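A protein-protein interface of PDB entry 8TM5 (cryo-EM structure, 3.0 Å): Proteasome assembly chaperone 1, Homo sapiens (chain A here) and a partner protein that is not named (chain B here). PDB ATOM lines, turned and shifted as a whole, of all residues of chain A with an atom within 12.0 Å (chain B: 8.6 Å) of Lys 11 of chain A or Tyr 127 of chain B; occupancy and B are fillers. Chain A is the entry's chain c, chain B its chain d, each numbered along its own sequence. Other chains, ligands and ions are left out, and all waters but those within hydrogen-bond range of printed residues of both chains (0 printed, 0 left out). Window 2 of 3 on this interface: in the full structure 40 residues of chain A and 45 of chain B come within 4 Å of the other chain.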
ATOM      1  N   ALA A   2      18.837 -31.024   8.814  1.00  0.00           N
ATOM      2  CA  ALA A   2      17.777 -31.110   9.857  1.00  0.00           C
ATOM      3  C   ALA A   2      17.772 -32.488  10.507  1.00  0.00           C
ATOM      4  O   ALA A   2      18.253 -32.658  11.627  1.00  0.00           O
ATOM      5  CB  ALA A   2      16.413 -30.803   9.254  1.00  0.00           C
ATOM      6  N   ALA A   3      17.230 -33.472   9.795  1.00  0.00           N
ATOM      7  CA  ALA A   3      17.126 -34.838  10.299  1.00  0.00           C
ATOM      8  C   ALA A   3      16.359 -34.868  11.617  1.00  0.00           C
ATOM      9  O   ALA A   3      16.680 -35.617  12.543  1.00  0.00           O
ATOM     10  CB  ALA A   3      18.510 -35.464  10.455  1.00  0.00           C
ATOM     11  N   THR A   4      15.322 -34.032  11.695  1.00  0.00           N
ATOM     12  CA  THR A   4      14.509 -33.981  12.907  1.00  0.00           C
ATOM     13  C   THR A   4      13.836 -35.322  13.171  1.00  0.00           C
ATOM     14  O   THR A   4      13.799 -35.791  14.314  1.00  0.00           O
ATOM     15  CB  THR A   4      13.463 -32.874  12.792  1.00  0.00           C
ATOM     16  OG1 THR A   4      14.117 -31.608  12.646  1.00  0.00           O
ATOM     17  CG2 THR A   4      12.578 -32.844  14.029  1.00  0.00           C
ATOM     18  N   PHE A   5      13.298 -35.951  12.128  1.00  0.00           N
ATOM     19  CA  PHE A   5      12.695 -37.270  12.239  1.00  0.00           C
ATOM     20  C   PHE A   5      13.290 -38.168  11.162  1.00  0.00           C
ATOM     21  O   PHE A   5      14.265 -37.812  10.494  1.00  0.00           O
ATOM     22  CB  PHE A   5      11.166 -37.196  12.140  1.00  0.00           C
ATOM     23  CG  PHE A   5      10.664 -36.605  10.855  1.00  0.00           C
ATOM     24  CD1 PHE A   5      10.522 -37.389   9.725  1.00  0.00           C
ATOM     25  CD2 PHE A   5      10.316 -35.269  10.785  1.00  0.00           C
ATOM     26  CE1 PHE A   5      10.054 -36.848   8.544  1.00  0.00           C
ATOM     27  CE2 PHE A   5       9.845 -34.725   9.611  1.00  0.00           C
ATOM     28  CZ  PHE A   5       9.715 -35.515   8.489  1.00  0.00           C
ATOM     29  N   PHE A   6      12.694 -39.347  10.997  1.00  0.00           N
ATOM     30  CA  PHE A   6      13.256 -40.385  10.143  1.00  0.00           C
ATOM     31  C   PHE A   6      13.436 -39.915   8.703  1.00  0.00           C
ATOM     32  O   PHE A   6      14.562 -39.877   8.196  1.00  0.00           O
ATOM     33  CB  PHE A   6      12.363 -41.627  10.179  1.00  0.00           C
ATOM     34  CG  PHE A   6      13.088 -42.905   9.878  1.00  0.00           C
ATOM     35  CD1 PHE A   6      14.127 -43.333  10.685  1.00  0.00           C
ATOM     36  CD2 PHE A   6      12.729 -43.680   8.790  1.00  0.00           C
ATOM     37  CE1 PHE A   6      14.793 -44.508  10.412  1.00  0.00           C
ATOM     38  CE2 PHE A   6      13.392 -44.856   8.513  1.00  0.00           C
ATOM     39  CZ  PHE A   6      14.425 -45.271   9.325  1.00  0.00           C
ATOM     40  N   GLY A   7      12.342 -39.557   8.038  1.00  0.00           N
ATOM     41  CA  GLY A   7      12.389 -39.272   6.617  1.00  0.00           C
ATOM     42  C   GLY A   7      12.550 -37.807   6.270  1.00  0.00           C
ATOM     43  O   GLY A   7      12.267 -37.405   5.137  1.00  0.00           O
ATOM     44  N   GLU A   8      13.000 -36.997   7.226  1.00  0.00           N
ATOM     45  CA  GLU A   8      13.212 -35.577   6.971  1.00  0.00           C
ATOM     46  C   GLU A   8      14.103 -35.353   5.758  1.00  0.00           C
ATOM     47  O   GLU A   8      15.277 -35.735   5.759  1.00  0.00           O
ATOM     48  CB  GLU A   8      13.821 -34.902   8.203  1.00  0.00           C
ATOM     49  CG  GLU A   8      13.870 -33.367   8.169  1.00  0.00           C
ATOM     50  CD  GLU A   8      12.554 -32.699   7.806  1.00  0.00           C
ATOM     51  OE1 GLU A   8      12.565 -31.473   7.569  1.00  0.00           O
ATOM     52  OE2 GLU A   8      11.510 -33.376   7.771  1.00  0.00           O
ATOM     53  N   VAL A   9      13.547 -34.735   4.717  1.00  0.00           N
ATOM     54  CA  VAL A   9      14.343 -34.348   3.560  1.00  0.00           C
ATOM     55  C   VAL A   9      15.238 -33.181   3.948  1.00  0.00           C
ATOM     56  O   VAL A   9      14.770 -32.175   4.499  1.00  0.00           O
ATOM     57  CB  VAL A   9      13.434 -33.987   2.377  1.00  0.00           C
ATOM     58  CG1 VAL A   9      14.241 -33.343   1.259  1.00  0.00           C
ATOM     59  CG2 VAL A   9      12.709 -35.222   1.869  1.00  0.00           C
ATOM     60  N   VAL A  10      16.530 -33.307   3.661  1.00  0.00           N
ATOM     61  CA  VAL A  10      17.523 -32.320   4.052  1.00  0.00           C
ATOM     62  C   VAL A  10      18.189 -31.777   2.795  1.00  0.00           C
ATOM     63  O   VAL A  10      18.000 -32.287   1.692  1.00  0.00           O
ATOM     64  CB  VAL A  10      18.572 -32.901   5.018  1.00  0.00           C
ATOM     65  CG1 VAL A  10      17.936 -33.211   6.360  1.00  0.00           C
ATOM     66  CG2 VAL A  10      19.211 -34.149   4.424  1.00  0.00           C
ATOM     67  N   LYS A  11      18.977 -30.720   2.979  1.00  0.00           N
ATOM     68  CA  LYS A  11      19.723 -30.107   1.893  1.00  0.00           C
ATOM     69  C   LYS A  11      21.149 -29.853   2.357  1.00  0.00           C
ATOM     70  O   LYS A  11      21.409 -29.624   3.541  1.00  0.00           O
ATOM     71  CB  LYS A  11      19.068 -28.801   1.427  1.00  0.00           C
ATOM     72  CG  LYS A  11      17.784 -29.012   0.640  1.00  0.00           C
ATOM     73  CD  LYS A  11      17.251 -27.709   0.061  1.00  0.00           C
ATOM     74  CE  LYS A  11      16.855 -26.719   1.146  1.00  0.00           C
ATOM     75  NZ  LYS A  11      15.864 -27.294   2.097  1.00  0.00           N
ATOM     76  N   ALA A  12      22.073 -29.897   1.407  1.00  0.00           N
ATOM     77  CA  ALA A  12      23.479 -29.769   1.756  1.00  0.00           C
ATOM     78  C   ALA A  12      23.843 -28.312   2.035  1.00  0.00           C
ATOM     79  O   ALA A  12      23.294 -27.399   1.410  1.00  0.00           O
ATOM     80  CB  ALA A  12      24.358 -30.299   0.628  1.00  0.00           C
ATOM     81  N   PRO A  13      24.759 -28.055   2.970  1.00  0.00           N
ATOM     82  CA  PRO A  13      25.282 -26.691   3.127  1.00  0.00           C
ATOM     83  C   PRO A  13      25.844 -26.173   1.812  1.00  0.00           C
ATOM     84  O   PRO A  13      26.454 -26.916   1.043  1.00  0.00           O
ATOM     85  CB  PRO A  13      26.383 -26.857   4.183  1.00  0.00           C
ATOM     86  CG  PRO A  13      26.148 -28.218   4.826  1.00  0.00           C
ATOM     87  CD  PRO A  13      24.903 -28.804   4.228  1.00  0.00           C
ATOM     88  N   CYS A  14      25.628 -24.885   1.555  1.00  0.00           N
ATOM     89  CA  CYS A  14      26.095 -24.247   0.326  1.00  0.00           C
ATOM     90  C   CYS A  14      27.276 -23.342   0.658  1.00  0.00           C
ATOM     91  O   CYS A  14      27.169 -22.441   1.494  1.00  0.00           O
ATOM     92  CB  CYS A  14      24.966 -23.467  -0.335  1.00  0.00           C
ATOM     93  SG  CYS A  14      25.420 -22.676  -1.892  1.00  0.00           S
ATOM     94  N   ARG A  15      28.412 -23.588   0.002  1.00  0.00           N
ATOM     95  CA  ARG A  15      29.591 -22.753   0.215  1.00  0.00           C
ATOM     96  C   ARG A  15      29.335 -21.315  -0.218  1.00  0.00           C
ATOM     97  O   ARG A  15      29.698 -20.366   0.486  1.00  0.00           O
ATOM     98  CB  ARG A  15      30.784 -23.326  -0.548  1.00  0.00           C
ATOM     99  CG  ARG A  15      31.448 -24.505   0.137  1.00  0.00           C
ATOM    100  CD  ARG A  15      32.634 -25.019  -0.655  1.00  0.00           C
ATOM    101  NE  ARG A  15      32.220 -25.767  -1.835  1.00  0.00           N
ATOM    102  CZ  ARG A  15      32.941 -25.892  -2.941  1.00  0.00           C
ATOM    103  NH1 ARG A  15      34.139 -25.339  -3.055  1.00  0.00           N
ATOM    104  NH2 ARG A  15      32.446 -26.588  -3.960  1.00  0.00           N
ATOM    105  N   ALA A  16      28.724 -21.135  -1.389  1.00  0.00           N
ATOM    106  CA  ALA A  16      28.482 -19.797  -1.909  1.00  0.00           C
ATOM    107  C   ALA A  16      27.417 -19.045  -1.125  1.00  0.00           C
ATOM    108  O   ALA A  16      27.332 -17.819  -1.245  1.00  0.00           O
ATOM    109  CB  ALA A  16      28.065 -19.876  -3.377  1.00  0.00           C
ATOM    110  N   GLY A  17      26.604 -19.742  -0.336  1.00  0.00           N
ATOM    111  CA  GLY A  17      25.479 -19.092   0.312  1.00  0.00           C
ATOM    112  C   GLY A  17      24.523 -18.450  -0.667  1.00  0.00           C
ATOM    113  O   GLY A  17      23.806 -17.512  -0.304  1.00  0.00           O
ATOM    114  N   THR A  18      24.492 -18.939  -1.908  1.00  0.00           N
ATOM    115  CA  THR A  18      23.681 -18.311  -2.945  1.00  0.00           C
ATOM    116  C   THR A  18      22.193 -18.379  -2.633  1.00  0.00           C
ATOM    117  O   THR A  18      21.430 -17.528  -3.102  1.00  0.00           O
ATOM    118  CB  THR A  18      23.947 -18.963  -4.305  1.00  0.00           C
ATOM    119  OG1 THR A  18      22.922 -18.581  -5.232  1.00  0.00           O
ATOM    120  CG2 THR A  18      23.967 -20.483  -4.195  1.00  0.00           C
ATOM    121  N   GLU A  19      21.755 -19.379  -1.866  1.00  0.00           N
ATOM    122  CA  GLU A  19      20.354 -19.433  -1.463  1.00  0.00           C
ATOM    123  C   GLU A  19      19.967 -18.236  -0.604  1.00  0.00           C
ATOM    124  O   GLU A  19      18.911 -17.633  -0.825  1.00  0.00           O
ATOM    125  CB  GLU A  19      20.078 -20.731  -0.706  1.00  0.00           C
ATOM    126  N   ASP A  20      20.810 -17.874   0.366  1.00  0.00           N
ATOM    127  CA  ASP A  20      20.524 -16.709   1.194  1.00  0.00           C
ATOM    128  C   ASP A  20      20.512 -15.434   0.361  1.00  0.00           C
ATOM    129  O   ASP A  20      19.660 -14.560   0.560  1.00  0.00           O
ATOM    130  CB  ASP A  20      21.550 -16.604   2.321  1.00  0.00           C
ATOM    131  N   GLU A  22      19.798 -15.173  -2.860  1.00  0.00           N
ATOM    132  CA  GLU A  22      18.577 -15.183  -3.658  1.00  0.00           C
ATOM    133  C   GLU A  22      17.369 -14.807  -2.812  1.00  0.00           C
ATOM    134  O   GLU A  22      16.493 -14.062  -3.268  1.00  0.00           O
ATOM    135  CB  GLU A  22      18.379 -16.559  -4.295  1.00  0.00           C
ATOM    136  N   GLU A  23      17.303 -15.314  -1.580  1.00  0.00           N
ATOM    137  CA  GLU A  23      16.225 -14.910  -0.683  1.00  0.00           C
ATOM    138  C   GLU A  23      16.263 -13.412  -0.414  1.00  0.00           C
ATOM    139  O   GLU A  23      15.214 -12.757  -0.406  1.00  0.00           O
ATOM    140  CB  GLU A  23      16.315 -15.687   0.631  1.00  0.00           C
ATOM    141  N   VAL B  24      26.266 -22.313  -6.566  1.00  0.00           N
ATOM    142  CA  VAL B  24      26.485 -23.697  -6.140  1.00  0.00           C
ATOM    143  C   VAL B  24      27.962 -24.062  -6.157  1.00  0.00           C
ATOM    144  O   VAL B  24      28.498 -24.488  -7.185  1.00  0.00           O
ATOM    145  CB  VAL B  24      25.690 -24.676  -7.023  1.00  0.00           C
ATOM    146  CG1 VAL B  24      25.632 -26.048  -6.369  1.00  0.00           C
ATOM    147  CG2 VAL B  24      24.290 -24.147  -7.279  1.00  0.00           C
ATOM    148  N   SER B 124      24.052 -24.228 -11.695  1.00  0.00           N
ATOM    149  CA  SER B 124      22.766 -24.495 -11.074  1.00  0.00           C
ATOM    150  C   SER B 124      22.848 -25.809 -10.305  1.00  0.00           C
ATOM    151  O   SER B 124      23.885 -26.474 -10.267  1.00  0.00           O
ATOM    152  CB  SER B 124      21.657 -24.531 -12.126  1.00  0.00           C
ATOM    153  OG  SER B 124      20.384 -24.657 -11.518  1.00  0.00           O
ATOM    154  N   HIS B 125      21.733 -26.185  -9.688  1.00  0.00           N
ATOM    155  CA  HIS B 125      21.700 -27.386  -8.868  1.00  0.00           C
ATOM    156  C   HIS B 125      21.444 -28.616  -9.726  1.00  0.00           C
ATOM    157  O   HIS B 125      20.480 -28.666 -10.494  1.00  0.00           O
ATOM    158  CB  HIS B 125      20.621 -27.265  -7.794  1.00  0.00           C
ATOM    159  CG  HIS B 125      21.036 -26.447  -6.613  1.00  0.00           C
ATOM    160  ND1 HIS B 125      22.182 -26.707  -5.894  1.00  0.00           N
ATOM    161  CD2 HIS B 125      20.460 -25.369  -6.028  1.00  0.00           C
ATOM    162  CE1 HIS B 125      22.293 -25.828  -4.915  1.00  0.00           C
ATOM    163  NE2 HIS B 125      21.261 -25.005  -4.973  1.00  0.00           N
ATOM    164  N   SER B 126      22.314 -29.615  -9.587  1.00  0.00           N
ATOM    165  CA  SER B 126      22.126 -30.885 -10.275  1.00  0.00           C
ATOM    166  C   SER B 126      20.893 -31.629  -9.785  1.00  0.00           C
ATOM    167  O   SER B 126      20.444 -32.562 -10.459  1.00  0.00           O
ATOM    168  CB  SER B 126      23.365 -31.766 -10.110  1.00  0.00           C
ATOM    169  OG  SER B 126      23.624 -32.038  -8.746  1.00  0.00           O
ATOM    170  N   TYR B 127      20.349 -31.248  -8.638  1.00  0.00           N
ATOM    171  CA  TYR B 127      19.034 -31.678  -8.194  1.00  0.00           C
ATOM    172  C   TYR B 127      18.043 -30.548  -8.458  1.00  0.00           C
ATOM    173  O   TYR B 127      18.398 -29.491  -8.988  1.00  0.00           O
ATOM    174  CB  TYR B 127      19.074 -32.096  -6.723  1.00  0.00           C
ATOM    175  CG  TYR B 127      19.053 -30.953  -5.740  1.00  0.00           C
ATOM    176  CD1 TYR B 127      20.176 -30.162  -5.542  1.00  0.00           C
ATOM    177  CD2 TYR B 127      17.923 -30.682  -4.987  1.00  0.00           C
ATOM    178  CE1 TYR B 127      20.163 -29.120  -4.639  1.00  0.00           C
ATOM    179  CE2 TYR B 127      17.903 -29.646  -4.080  1.00  0.00           C
ATOM    180  CZ  TYR B 127      19.024 -28.867  -3.910  1.00  0.00           C
ATOM    181  OH  TYR B 127      19.005 -27.832  -3.005  1.00  0.00           O
ATOM    182  N   GLN B 128      16.783 -30.772  -8.090  1.00  0.00           N
ATOM    183  CA  GLN B 128      15.686 -29.937  -8.580  1.00  0.00           C
ATOM    184  C   GLN B 128      15.634 -29.979 -10.103  1.00  0.00           C
ATOM    185  O   GLN B 128      15.254 -29.007 -10.759  1.00  0.00           O
ATOM    186  CB  GLN B 128      15.801 -28.492  -8.091  1.00  0.00           C
ATOM    187  CG  GLN B 128      16.494 -28.308  -6.757  1.00  0.00           C
ATOM    188  CD  GLN B 128      16.260 -26.925  -6.183  1.00  0.00           C
ATOM    189  OE1 GLN B 128      15.815 -26.018  -6.885  1.00  0.00           O
ATOM    190  NE2 GLN B 128      16.551 -26.758  -4.899  1.00  0.00           N
ATOM    191  N   ARG B 129      16.027 -31.116 -10.668  1.00  0.00           N
ATOM    192  CA  ARG B 129      16.105 -31.305 -12.108  1.00  0.00           C
ATOM    193  C   ARG B 129      14.995 -32.242 -12.554  1.00  0.00           C
ATOM    194  O   ARG B 129      14.751 -33.272 -11.916  1.00  0.00           O
ATOM    195  CB  ARG B 129      17.466 -31.872 -12.511  1.00  0.00           C
ATOM    196  CG  ARG B 129      18.476 -30.813 -12.903  1.00  0.00           C
ATOM    197  CD  ARG B 129      19.789 -31.418 -13.379  1.00  0.00           C
ATOM    198  NE  ARG B 129      20.085 -32.691 -12.733  1.00  0.00           N
ATOM    199  CZ  ARG B 129      20.923 -33.600 -13.213  1.00  0.00           C
ATOM    200  NH1 ARG B 129      21.580 -33.406 -14.345  1.00  0.00           N
ATOM    201  NH2 ARG B 129      21.109 -34.730 -12.538  1.00  0.00           N
ATOM    202  N   ASN B 130      14.327 -31.881 -13.644  1.00  0.00           N
ATOM    203  CA  ASN B 130      13.309 -32.747 -14.213  1.00  0.00           C
ATOM    204  C   ASN B 130      13.948 -34.021 -14.752  1.00  0.00           C
ATOM    205  O   ASN B 130      15.163 -34.105 -14.949  1.00  0.00           O
ATOM    206  CB  ASN B 130      12.562 -32.034 -15.337  1.00  0.00           C
ATOM    207  CG  ASN B 130      11.980 -30.708 -14.901  1.00  0.00           C
ATOM    208  OD1 ASN B 130      11.765 -30.472 -13.712  1.00  0.00           O
ATOM    209  ND2 ASN B 130      11.726 -29.829 -15.862  1.00  0.00           N
ATOM    210  N   GLN B 133      15.750 -33.036 -17.712  1.00  0.00           N
ATOM    211  CA  GLN B 133      17.001 -32.360 -17.380  1.00  0.00           C
ATOM    212  C   GLN B 133      18.041 -33.347 -16.868  1.00  0.00           C
ATOM    213  O   GLN B 133      19.217 -33.267 -17.241  1.00  0.00           O
ATOM    214  CB  GLN B 133      16.752 -31.265 -16.343  1.00  0.00           C
ATOM    215  CG  GLN B 133      15.785 -30.188 -16.795  1.00  0.00           C
ATOM    216  CD  GLN B 133      15.559 -29.132 -15.733  1.00  0.00           C
ATOM    217  OE1 GLN B 133      14.697 -29.281 -14.868  1.00  0.00           O
ATOM    218  NE2 GLN B 133      16.336 -28.058 -15.792  1.00  0.00           N
ATOM    219  N   LEU B 134      17.628 -34.283 -16.014  1.00  0.00           N
ATOM    220  CA  LEU B 134      18.558 -35.276 -15.491  1.00  0.00           C
ATOM    221  C   LEU B 134      19.108 -36.146 -16.613  1.00  0.00           C
ATOM    222  O   LEU B 134      20.282 -36.531 -16.604  1.00  0.00           O
ATOM    223  CB  LEU B 134      17.859 -36.127 -14.426  1.00  0.00           C
ATOM    224  CG  LEU B 134      18.503 -37.449 -13.993  1.00  0.00           C
ATOM    225  CD1 LEU B 134      18.004 -37.840 -12.610  1.00  0.00           C
ATOM    226  CD2 LEU B 134      18.217 -38.571 -14.987  1.00  0.00           C
ATOM    227  N   MET B 163      18.458 -22.986 -20.699  1.00  0.00           N
ATOM    228  CA  MET B 163      17.942 -23.213 -19.357  1.00  0.00           C
ATOM    229  C   MET B 163      16.422 -23.240 -19.380  1.00  0.00           C
ATOM    230  O   MET B 163      15.780 -22.370 -19.974  1.00  0.00           O
ATOM    231  CB  MET B 163      18.442 -22.115 -18.415  1.00  0.00           C
ATOM    232  CG  MET B 163      18.062 -22.307 -16.953  1.00  0.00           C
ATOM    233  SD  MET B 163      18.641 -23.869 -16.262  1.00  0.00           S
ATOM    234  CE  MET B 163      17.135 -24.498 -15.527  1.00  0.00           C
ATOM    235  N   ILE B 181      17.319 -19.997 -11.917  1.00  0.00           N
ATOM    236  CA  ILE B 181      18.571 -20.745 -11.849  1.00  0.00           C
ATOM    237  C   ILE B 181      18.760 -21.205 -10.410  1.00  0.00           C
ATOM    238  O   ILE B 181      19.441 -20.523  -9.630  1.00  0.00           O
ATOM    239  CB  ILE B 181      19.761 -19.899 -12.326  1.00  0.00           C
ATOM    240  CG1 ILE B 181      19.547 -19.449 -13.772  1.00  0.00           C
ATOM    241  CG2 ILE B 181      21.055 -20.690 -12.212  1.00  0.00           C
ATOM    242  CD1 ILE B 181      19.152 -18.000 -13.902  1.00  0.00           C
ATOM    243  N   PRO B 182      18.169 -22.333 -10.008  1.00  0.00           N
ATOM    244  CA  PRO B 182      18.347 -22.813  -8.631  1.00  0.00           C
ATOM    245  C   PRO B 182      19.805 -22.828  -8.204  1.00  0.00           C
ATOM    246  O   PRO B 182      20.641 -23.479  -8.840  1.00  0.00           O
ATOM    247  CB  PRO B 182      17.764 -24.229  -8.682  1.00  0.00           C
ATOM    248  CG  PRO B 182      16.732 -24.162  -9.747  1.00  0.00           C
ATOM    249  CD  PRO B 182      17.252 -23.193 -10.777  1.00  0.00           C
ATOM    250  N   GLY B 183      20.120 -22.115  -7.128  1.00  0.00           N
ATOM    251  CA  GLY B 183      21.491 -21.991  -6.683  1.00  0.00           C
ATOM    252  C   GLY B 183      22.332 -21.037  -7.496  1.00  0.00           C
ATOM    253  O   GLY B 183      23.564 -21.115  -7.435  1.00  0.00           O
ATOM    254  N   PHE B 207      24.645 -27.844 -14.600  1.00  0.00           N
ATOM    255  CA  PHE B 207      23.985 -28.482 -13.469  1.00  0.00           C
ATOM    256  C   PHE B 207      25.011 -29.279 -12.676  1.00  0.00           C
ATOM    257  O   PHE B 207      25.657 -30.180 -13.222  1.00  0.00           O
ATOM    258  CB  PHE B 207      22.850 -29.386 -13.948  1.00  0.00           C
ATOM    259  CG  PHE B 207      21.668 -28.639 -14.495  1.00  0.00           C
ATOM    260  CD1 PHE B 207      20.996 -27.713 -13.717  1.00  0.00           C
ATOM    261  CD2 PHE B 207      21.229 -28.863 -15.788  1.00  0.00           C
ATOM    262  CE1 PHE B 207      19.911 -27.026 -14.218  1.00  0.00           C
ATOM    263  CE2 PHE B 207      20.143 -28.179 -16.292  1.00  0.00           C
ATOM    264  CZ  PHE B 207      19.484 -27.260 -15.507  1.00  0.00           C
ATOM    265  N   VAL B 208      25.175 -28.961 -11.391  1.00  0.00           N
ATOM    266  CA  VAL B 208      26.252 -29.520 -10.586  1.00  0.00           C
ATOM    267  C   VAL B 208      25.808 -29.643  -9.135  1.00  0.00           C
ATOM    268  O   VAL B 208      24.870 -28.983  -8.687  1.00  0.00           O
ATOM    269  CB  VAL B 208      27.528 -28.653 -10.675  1.00  0.00           C
ATOM    270  CG1 VAL B 208      27.343 -27.369  -9.893  1.00  0.00           C
ATOM    271  CG2 VAL B 208      28.735 -29.415 -10.172  1.00  0.00           C
ATOM    272  N   SER B 209      26.504 -30.510  -8.406  1.00  0.00           N
ATOM    273  CA  SER B 209      26.390 -30.617  -6.961  1.00  0.00           C
ATOM    274  C   SER B 209      27.733 -30.264  -6.336  1.00  0.00           C
ATOM    275  O   SER B 209      28.794 -30.500  -6.921  1.00  0.00           O
ATOM    276  CB  SER B 209      25.963 -32.025  -6.533  1.00  0.00           C
ATOM    277  OG  SER B 209      26.639 -33.014  -7.290  1.00  0.00           O
ATOM    278  N   GLU B 210      27.682 -29.698  -5.137  1.00  0.00           N
ATOM    279  CA  GLU B 210      28.882 -29.197  -4.487  1.00  0.00           C
ATOM    280  C   GLU B 210      29.839 -30.338  -4.157  1.00  0.00           C
ATOM    281  O   GLU B 210      29.460 -31.510  -4.099  1.00  0.00           O
ATOM    282  CB  GLU B 210      28.527 -28.427  -3.216  1.00  0.00           C
ATOM    283  CG  GLU B 210      27.959 -27.041  -3.484  1.00  0.00           C
ATOM    284  CD  GLU B 210      28.270 -26.050  -2.377  1.00  0.00           C
ATOM    285  OE1 GLU B 210      27.707 -24.935  -2.405  1.00  0.00           O
ATOM    286  OE2 GLU B 210      29.073 -26.381  -1.479  1.00  0.00           O
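Of the 21 printed residues of chain A, 5 touch a printed residue of chain B. Printed residues of chain A that touch a printed residue of chain B: Lys 11, Pro 13, Cys 14, Arg 15 and Thr 18. Along chain A the printed residues that touch a printed residue of chain B span positions 11 to 18. Of the 18 printed residues of chain B, 4 touch a printed residue of chain A. Among the printed residues, 6 pairs touch across the chains. Among the printed residues, Asp or Glu carboxylates within 4 Å of a Lys or Arg side-chain nitrogen of the other chain: Arg 15 of chain A with Glu 210 of chain B (3.2 Å).
The side-chain sulfur (SG) of Cys 14 of chain A sits close to the backbone NH (N) of Ala 16 of chain A, 3.7 Å away. The backbone NH (N) of Val 24 of chain B sits at hydrogen-bond distance from the backbone carbonyl oxygen (O) of Gly 183 of chain B (3.1 Å). The side-chain hydroxyl (OH) of Tyr 127 of chain B is in hydrogen-bond range of the side-chain amide nitrogen (NE2) of Gln 128 of chain B, 3.3 Å away. SG of Cys 14 of chain A is in hydrogen-bond range of N of Gly 17 of chain A (3.5 Å).
Among the printed residues, pairs that only touch across the chains: Lys 11 of chain A with Tyr 127 of chain B, Pro 13 of chain A with Glu 210 of chain B and Thr 18 of chain A with Val 24 of chain B.
The side-chain sulfur of Cys 14 of chain A sits close to the side-chain carboxylate of Glu 210 of chain B (3.3 Å). The side-chain hydroxyl (OG1) of Thr 18 of chain A lies close to the backbone carbonyl oxygen (O) of Gly 183 of chain B (3.4 Å). OE2 of Glu 210 of chain B is in salt-bridge range of NE of Arg 15 of chain A (3.2 Å).
Val 10 of chain A touches none of the printed residues of chain B. Of the printed residues of chain B, Lys 11 of chain A touches Tyr 127 (3.5 Å). No residue of chain B comes within 4 Å of Ala 12 of chain A. Printed residues of chain B within 4 Å of Pro 13 of chain A: Glu 210 (3.7 Å). Printed residues of chain B within 4 Å of Cys 14 of chain A: Glu 210 (3.2 Å). Printed residues of chain B within 4 Å of Arg 15 of chain A: Glu 210 (2.8 Å). Ala 16 of chain A touches none of the printed residues of chain B. Printed residues of chain B within 4 Å of Thr 18 of chain A: Val 24 (3.8 Å) and Gly 183 (3.3 Å). No residue of chain A comes within 4 Å of His 125 of chain B. No residue of chain A comes within 4 Å of Ser 126 of chain B. Of chain A, only Lys 11 (3.5 Å) comes within 4 Å of Tyr 127 of chain B. No residue of chain A comes within 4 Å of Arg 129 of chain B. No residue of chain A comes within 4 Å of Pro 182 of chain B. Printed residues of chain A within 4 Å of Gly 183 of chain B: Thr 18.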
